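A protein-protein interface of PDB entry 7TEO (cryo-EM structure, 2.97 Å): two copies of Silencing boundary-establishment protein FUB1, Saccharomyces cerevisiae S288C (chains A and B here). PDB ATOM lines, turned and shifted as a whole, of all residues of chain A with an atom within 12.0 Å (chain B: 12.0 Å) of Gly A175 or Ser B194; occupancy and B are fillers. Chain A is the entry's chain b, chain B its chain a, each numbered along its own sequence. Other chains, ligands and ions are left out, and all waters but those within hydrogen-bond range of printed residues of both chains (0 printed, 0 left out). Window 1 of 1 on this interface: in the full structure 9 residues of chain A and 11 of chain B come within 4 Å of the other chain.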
ATOM      1  N   PRO A 162      11.844  18.519  23.321  1.00  0.00           N
ATOM      2  CA  PRO A 162      10.958  17.809  22.394  1.00  0.00           C
ATOM      3  C   PRO A 162      10.199  16.688  23.086  1.00  0.00           C
ATOM      4  O   PRO A 162      10.659  16.109  24.073  1.00  0.00           O
ATOM      5  CB  PRO A 162      11.919  17.255  21.332  1.00  0.00           C
ATOM      6  CG  PRO A 162      13.209  17.994  21.533  1.00  0.00           C
ATOM      7  CD  PRO A 162      13.261  18.308  22.988  1.00  0.00           C
ATOM      8  N   ALA A 163       9.020  16.387  22.552  1.00  0.00           N
ATOM      9  CA  ALA A 163       8.207  15.303  23.082  1.00  0.00           C
ATOM     10  C   ALA A 163       8.738  13.956  22.606  1.00  0.00           C
ATOM     11  O   ALA A 163       9.153  13.797  21.455  1.00  0.00           O
ATOM     12  CB  ALA A 163       6.748  15.466  22.658  1.00  0.00           C
ATOM     13  N   GLY A 164       8.717  12.979  23.508  1.00  0.00           N
ATOM     14  CA  GLY A 164       9.229  11.667  23.184  1.00  0.00           C
ATOM     15  C   GLY A 164       8.323  10.904  22.237  1.00  0.00           C
ATOM     16  O   GLY A 164       7.141  11.203  22.072  1.00  0.00           O
ATOM     17  N   GLY A 165       8.905   9.891  21.600  1.00  0.00           N
ATOM     18  CA  GLY A 165       8.139   9.055  20.699  1.00  0.00           C
ATOM     19  C   GLY A 165       7.085   8.247  21.432  1.00  0.00           C
ATOM     20  O   GLY A 165       7.213   7.936  22.617  1.00  0.00           O
ATOM     21  N   TYR A 166       6.020   7.905  20.706  1.00  0.00           N
ATOM     22  CA  TYR A 166       4.908   7.187  21.320  1.00  0.00           C
ATOM     23  C   TYR A 166       5.330   5.812  21.824  1.00  0.00           C
ATOM     24  O   TYR A 166       4.715   5.281  22.755  1.00  0.00           O
ATOM     25  CB  TYR A 166       3.750   7.074  20.325  1.00  0.00           C
ATOM     26  CG  TYR A 166       3.852   5.931  19.337  1.00  0.00           C
ATOM     27  CD1 TYR A 166       3.383   4.664  19.658  1.00  0.00           C
ATOM     28  CD2 TYR A 166       4.401   6.124  18.077  1.00  0.00           C
ATOM     29  CE1 TYR A 166       3.469   3.622  18.755  1.00  0.00           C
ATOM     30  CE2 TYR A 166       4.490   5.087  17.169  1.00  0.00           C
ATOM     31  CZ  TYR A 166       4.022   3.839  17.515  1.00  0.00           C
ATOM     32  OH  TYR A 166       4.104   2.801  16.616  1.00  0.00           O
ATOM     33  N   ALA A 167       6.367   5.222  21.229  1.00  0.00           N
ATOM     34  CA  ALA A 167       6.850   3.903  21.623  1.00  0.00           C
ATOM     35  C   ALA A 167       8.262   3.949  22.194  1.00  0.00           C
ATOM     36  O   ALA A 167       8.956   2.928  22.201  1.00  0.00           O
ATOM     37  CB  ALA A 167       6.797   2.944  20.433  1.00  0.00           C
ATOM     38  N   ASP A 168       8.704   5.115  22.673  1.00  0.00           N
ATOM     39  CA  ASP A 168      10.033   5.207  23.268  1.00  0.00           C
ATOM     40  C   ASP A 168      10.168   4.286  24.474  1.00  0.00           C
ATOM     41  O   ASP A 168      11.283   3.877  24.817  1.00  0.00           O
ATOM     42  CB  ASP A 168      10.332   6.651  23.666  1.00  0.00           C
ATOM     43  CG  ASP A 168      10.716   7.515  22.480  1.00  0.00           C
ATOM     44  OD1 ASP A 168      10.867   6.970  21.365  1.00  0.00           O
ATOM     45  OD2 ASP A 168      10.870   8.742  22.661  1.00  0.00           O
ATOM     46  N   GLY A 169       9.056   3.954  25.130  1.00  0.00           N
ATOM     47  CA  GLY A 169       9.117   3.017  26.237  1.00  0.00           C
ATOM     48  C   GLY A 169       9.592   1.642  25.815  1.00  0.00           C
ATOM     49  O   GLY A 169      10.301   0.967  26.566  1.00  0.00           O
ATOM     50  N   ASP A 170       9.213   1.208  24.614  1.00  0.00           N
ATOM     51  CA  ASP A 170       9.655  -0.076  24.086  1.00  0.00           C
ATOM     52  C   ASP A 170      11.013   0.003  23.404  1.00  0.00           C
ATOM     53  O   ASP A 170      11.639  -1.037  23.180  1.00  0.00           O
ATOM     54  CB  ASP A 170       8.620  -0.609  23.095  1.00  0.00           C
ATOM     55  CG  ASP A 170       8.974  -1.977  22.566  1.00  0.00           C
ATOM     56  OD1 ASP A 170       8.696  -2.979  23.257  1.00  0.00           O
ATOM     57  OD2 ASP A 170       9.532  -2.052  21.452  1.00  0.00           O
ATOM     58  N   LEU A 171      11.479   1.204  23.071  1.00  0.00           N
ATOM     59  CA  LEU A 171      12.728   1.371  22.337  1.00  0.00           C
ATOM     60  C   LEU A 171      13.939   1.477  23.257  1.00  0.00           C
ATOM     61  O   LEU A 171      15.032   1.035  22.886  1.00  0.00           O
ATOM     62  CB  LEU A 171      12.637   2.604  21.436  1.00  0.00           C
ATOM     63  CG  LEU A 171      13.847   2.891  20.549  1.00  0.00           C
ATOM     64  CD1 LEU A 171      14.088   1.770  19.564  1.00  0.00           C
ATOM     65  CD2 LEU A 171      13.653   4.205  19.807  1.00  0.00           C
ATOM     66  N   TYR A 172      13.776   2.061  24.445  1.00  0.00           N
ATOM     67  CA  TYR A 172      14.870   2.174  25.393  1.00  0.00           C
ATOM     68  C   TYR A 172      14.483   1.537  26.725  1.00  0.00           C
ATOM     69  O   TYR A 172      13.313   1.588  27.114  1.00  0.00           O
ATOM     70  CB  TYR A 172      15.256   3.644  25.606  1.00  0.00           C
ATOM     71  CG  TYR A 172      15.497   4.383  24.308  1.00  0.00           C
ATOM     72  CD1 TYR A 172      16.663   4.189  23.582  1.00  0.00           C
ATOM     73  CD2 TYR A 172      14.553   5.266  23.803  1.00  0.00           C
ATOM     74  CE1 TYR A 172      16.885   4.855  22.393  1.00  0.00           C
ATOM     75  CE2 TYR A 172      14.765   5.939  22.614  1.00  0.00           C
ATOM     76  CZ  TYR A 172      15.932   5.729  21.913  1.00  0.00           C
ATOM     77  OH  TYR A 172      16.149   6.395  20.729  1.00  0.00           O
ATOM     78  N   PRO A 173      15.435   0.933  27.445  1.00  0.00           N
ATOM     79  CA  PRO A 173      15.052   0.131  28.624  1.00  0.00           C
ATOM     80  C   PRO A 173      14.216   0.879  29.649  1.00  0.00           C
ATOM     81  O   PRO A 173      13.141   0.399  30.028  1.00  0.00           O
ATOM     82  CB  PRO A 173      16.411  -0.301  29.187  1.00  0.00           C
ATOM     83  CG  PRO A 173      17.272  -0.392  27.986  1.00  0.00           C
ATOM     84  CD  PRO A 173      16.874   0.793  27.151  1.00  0.00           C
ATOM     85  N   VAL A 174      14.670   2.042  30.110  1.00  0.00           N
ATOM     86  CA  VAL A 174      13.945   2.776  31.141  1.00  0.00           C
ATOM     87  C   VAL A 174      12.980   3.754  30.485  1.00  0.00           C
ATOM     88  O   VAL A 174      12.404   4.619  31.154  1.00  0.00           O
ATOM     89  CB  VAL A 174      14.913   3.503  32.094  1.00  0.00           C
ATOM     90  CG1 VAL A 174      15.639   2.498  32.980  1.00  0.00           C
ATOM     91  CG2 VAL A 174      15.903   4.362  31.315  1.00  0.00           C
ATOM     92  N   GLY A 175      12.792   3.621  29.173  1.00  0.00           N
ATOM     93  CA  GLY A 175      11.849   4.438  28.445  1.00  0.00           C
ATOM     94  C   GLY A 175      12.333   5.826  28.098  1.00  0.00           C
ATOM     95  O   GLY A 175      11.613   6.557  27.406  1.00  0.00           O
ATOM     96  N   THR A 176      13.521   6.216  28.546  1.00  0.00           N
ATOM     97  CA  THR A 176      14.088   7.519  28.232  1.00  0.00           C
ATOM     98  C   THR A 176      15.290   7.339  27.315  1.00  0.00           C
ATOM     99  O   THR A 176      16.183   6.536  27.605  1.00  0.00           O
ATOM    100  CB  THR A 176      14.504   8.258  29.505  1.00  0.00           C
ATOM    101  OG1 THR A 176      15.509   7.503  30.193  1.00  0.00           O
ATOM    102  CG2 THR A 176      13.307   8.466  30.425  1.00  0.00           C
ATOM    103  N   SER A 177      15.309   8.088  26.212  1.00  0.00           N
ATOM    104  CA  SER A 177      16.458   8.066  25.319  1.00  0.00           C
ATOM    105  C   SER A 177      17.715   8.604  25.986  1.00  0.00           C
ATOM    106  O   SER A 177      18.815   8.383  25.467  1.00  0.00           O
ATOM    107  CB  SER A 177      16.158   8.875  24.056  1.00  0.00           C
ATOM    108  OG  SER A 177      17.182   8.708  23.091  1.00  0.00           O
ATOM    109  N   HIS A 178      17.577   9.298  27.111  1.00  0.00           N
ATOM    110  CA  HIS A 178      18.691   9.835  27.871  1.00  0.00           C
ATOM    111  C   HIS A 178      18.580   9.370  29.314  1.00  0.00           C
ATOM    112  O   HIS A 178      17.472   9.161  29.817  1.00  0.00           O
ATOM    113  CB  HIS A 178      18.700  11.369  27.824  1.00  0.00           C
ATOM    114  CG  HIS A 178      18.560  11.930  26.443  1.00  0.00           C
ATOM    115  ND1 HIS A 178      19.574  11.880  25.510  1.00  0.00           N
ATOM    116  CD2 HIS A 178      17.521  12.553  25.836  1.00  0.00           C
ATOM    117  CE1 HIS A 178      19.166  12.447  24.389  1.00  0.00           C
ATOM    118  NE2 HIS A 178      17.924  12.864  24.560  1.00  0.00           N
ATOM    119  N   PRO A 179      19.714   9.205  30.014  1.00  0.00           N
ATOM    120  CA  PRO A 179      19.668   8.707  31.393  1.00  0.00           C
ATOM    121  C   PRO A 179      19.016   9.694  32.357  1.00  0.00           C
ATOM    122  O   PRO A 179      19.624  10.720  32.662  1.00  0.00           O
ATOM    123  CB  PRO A 179      21.144   8.500  31.739  1.00  0.00           C
ATOM    124  CG  PRO A 179      21.871   9.451  30.858  1.00  0.00           C
ATOM    125  CD  PRO A 179      21.091   9.495  29.579  1.00  0.00           C
ATOM    126  N   TYR B 149       0.310  12.011  43.800  1.00  0.00           N
ATOM    127  CA  TYR B 149       0.098  10.881  44.699  1.00  0.00           C
ATOM    128  C   TYR B 149       0.223  11.401  46.126  1.00  0.00           C
ATOM    129  O   TYR B 149       1.315  11.372  46.713  1.00  0.00           O
ATOM    130  CB  TYR B 149       1.098   9.767  44.402  1.00  0.00           C
ATOM    131  CG  TYR B 149       1.125   9.412  42.933  1.00  0.00           C
ATOM    132  CD1 TYR B 149       0.005   8.879  42.309  1.00  0.00           C
ATOM    133  CD2 TYR B 149       2.258   9.636  42.166  1.00  0.00           C
ATOM    134  CE1 TYR B 149       0.019   8.567  40.965  1.00  0.00           C
ATOM    135  CE2 TYR B 149       2.281   9.327  40.820  1.00  0.00           C
ATOM    136  CZ  TYR B 149       1.159   8.794  40.225  1.00  0.00           C
ATOM    137  OH  TYR B 149       1.178   8.483  38.884  1.00  0.00           O
ATOM    138  N   SER B 194       8.959   6.251  28.791  1.00  0.00           N
ATOM    139  CA  SER B 194       7.540   6.394  29.092  1.00  0.00           C
ATOM    140  C   SER B 194       6.861   5.034  29.212  1.00  0.00           C
ATOM    141  O   SER B 194       7.436   4.011  28.844  1.00  0.00           O
ATOM    142  CB  SER B 194       6.848   7.227  28.016  1.00  0.00           C
ATOM    143  OG  SER B 194       6.708   6.490  26.812  1.00  0.00           O
ATOM    144  N   GLN B 195       5.635   5.027  29.733  1.00  0.00           N
ATOM    145  CA  GLN B 195       4.856   3.802  29.837  1.00  0.00           C
ATOM    146  C   GLN B 195       4.317   3.328  28.495  1.00  0.00           C
ATOM    147  O   GLN B 195       3.931   2.161  28.378  1.00  0.00           O
ATOM    148  CB  GLN B 195       3.702   3.996  30.822  1.00  0.00           C
ATOM    149  CG  GLN B 195       2.778   2.788  30.972  1.00  0.00           C
ATOM    150  CD  GLN B 195       3.528   1.515  31.302  1.00  0.00           C
ATOM    151  OE1 GLN B 195       3.355   0.490  30.644  1.00  0.00           O
ATOM    152  NE2 GLN B 195       4.363   1.572  32.332  1.00  0.00           N
ATOM    153  N   GLY B 196       4.283   4.194  27.485  1.00  0.00           N
ATOM    154  CA  GLY B 196       3.772   3.811  26.181  1.00  0.00           C
ATOM    155  C   GLY B 196       4.549   2.636  25.617  1.00  0.00           C
ATOM    156  O   GLY B 196       5.792   2.655  25.599  1.00  0.00           O
ATOM    157  N   GLY B 197       3.838   1.609  25.158  1.00  0.00           N
ATOM    158  CA  GLY B 197       4.458   0.407  24.644  1.00  0.00           C
ATOM    159  C   GLY B 197       4.624   0.425  23.135  1.00  0.00           C
ATOM    160  O   GLY B 197       4.613   1.469  22.482  1.00  0.00           O
ATOM    161  N   MET B 198       4.791  -0.776  22.582  1.00  0.00           N
ATOM    162  CA  MET B 198       5.011  -0.936  21.153  1.00  0.00           C
ATOM    163  C   MET B 198       3.780  -0.589  20.326  1.00  0.00           C
ATOM    164  O   MET B 198       3.923  -0.121  19.190  1.00  0.00           O
ATOM    165  CB  MET B 198       5.432  -2.375  20.862  1.00  0.00           C
ATOM    166  CG  MET B 198       5.766  -2.658  19.419  1.00  0.00           C
ATOM    167  SD  MET B 198       6.334  -4.350  19.223  1.00  0.00           S
ATOM    168  CE  MET B 198       6.550  -4.437  17.453  1.00  0.00           C
ATOM    169  N   ILE B 199       2.582  -0.811  20.859  1.00  0.00           N
ATOM    170  CA  ILE B 199       1.335  -0.614  20.133  1.00  0.00           C
ATOM    171  C   ILE B 199       0.685   0.664  20.636  1.00  0.00           C
ATOM    172  O   ILE B 199       0.513   0.846  21.848  1.00  0.00           O
ATOM    173  CB  ILE B 199       0.391  -1.817  20.303  1.00  0.00           C
ATOM    174  CG1 ILE B 199       0.890  -3.009  19.480  1.00  0.00           C
ATOM    175  CG2 ILE B 199      -1.030  -1.448  19.902  1.00  0.00           C
ATOM    176  CD1 ILE B 199       0.717  -2.853  17.977  1.00  0.00           C
ATOM    177  N   PHE B 200       0.331   1.547  19.711  1.00  0.00           N
ATOM    178  CA  PHE B 200      -0.281   2.813  20.078  1.00  0.00           C
ATOM    179  C   PHE B 200      -1.739   2.583  20.455  1.00  0.00           C
ATOM    180  O   PHE B 200      -2.442   1.784  19.832  1.00  0.00           O
ATOM    181  CB  PHE B 200      -0.199   3.802  18.916  1.00  0.00           C
ATOM    182  CG  PHE B 200      -0.782   5.153  19.220  1.00  0.00           C
ATOM    183  CD1 PHE B 200      -0.733   5.671  20.504  1.00  0.00           C
ATOM    184  CD2 PHE B 200      -1.382   5.905  18.223  1.00  0.00           C
ATOM    185  CE1 PHE B 200      -1.260   6.913  20.786  1.00  0.00           C
ATOM    186  CE2 PHE B 200      -1.915   7.148  18.503  1.00  0.00           C
ATOM    187  CZ  PHE B 200      -1.853   7.650  19.786  1.00  0.00           C
ATOM    188  N   ASP B 201      -2.188   3.288  21.483  1.00  0.00           N
ATOM    189  CA  ASP B 201      -3.582   3.273  21.892  1.00  0.00           C
ATOM    190  C   ASP B 201      -4.000   4.692  22.243  1.00  0.00           C
ATOM    191  O   ASP B 201      -3.162   5.512  22.634  1.00  0.00           O
ATOM    192  CB  ASP B 201      -3.815   2.344  23.091  1.00  0.00           C
ATOM    193  CG  ASP B 201      -2.973   2.724  24.290  1.00  0.00           C
ATOM    194  OD1 ASP B 201      -3.334   2.332  25.420  1.00  0.00           O
ATOM    195  OD2 ASP B 201      -1.951   3.416  24.105  1.00  0.00           O
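Tyr A166 touches Gly B196. Tyr A166 touches Gly B197 (O to O, 3.8 Å). Met B198 touches Tyr A166. Tyr A166 touches Phe B200. CB of Ala A167 touches O of Gly B197, at 3.3 Å. Gly A169 touches Ser B194. Gly B196 touches Gly A169. Asp A170 touches Gly B196. Met B198 touches Asp A170.
The backbone NH (N) of Ser B194 lies within hydrogen-bond range of the backbone carbonyl oxygen (O) of Gly A175, 3.0 Å away.
No residue of chain B comes within 4 Å of Gly A164. No residue of chain B comes within 4 Å of Gly A165. Of the printed residues of chain B, Tyr A166 touches Gly B196, Gly B197, Met B198 and Phe B200. Ala A167 touches one residue of chain B. Of chain B, only Ser B194 and Gly B196 come within 4 Å of Gly A169. Of the printed residues of chain B, Asp A170 touches Gly B196 (3.8 Å) and Met B198 (3.9 Å). Leu A171 touches none of the printed residues of chain B. Pro A173 touches none of the printed residues of chain B. No residue of chain B comes within 4 Å of Val A174. Of chain B, only Ser B194 comes within 4 Å of Gly A175. No residue of chain B comes within 4 Å of Thr A176. No residue of chain B comes within 4 Å of Ser A177. His A178 touches none of the printed residues of chain B. Ser B194 touches two residues of chain A. Of chain A, only Tyr A166, Gly A169 and Asp A170 come within 4 Å of Gly B196. Printed residues of chain A within 4 Å of Gly B197: Tyr A166 (3.8 Å) and Ala A167 (3.3 Å). Of the printed residues of chain A, Met B198 touches Tyr A166 and Asp A170. Of the printed residues of chain A, Phe B200 touches Tyr A166. The nearest residue of chain B that does not touch Gly A175 is Gln B195 (6.4 Å).
Along chain B the printed residues that touch a printed residue of chain A span positions 194 to 200. Along chain A the printed residues that touch a printed residue of chain B span positions 166 to 175. Among the printed residues, 10 pairs touch across the chains. Among the printed residues, no Asp or Glu carboxylate lies within 4 Å of a Lys or Arg side-chain nitrogen of the other chain.
N of Gly B196 sits close to OG of Ser B194 (3.4 Å).
No position is printed for both chains.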
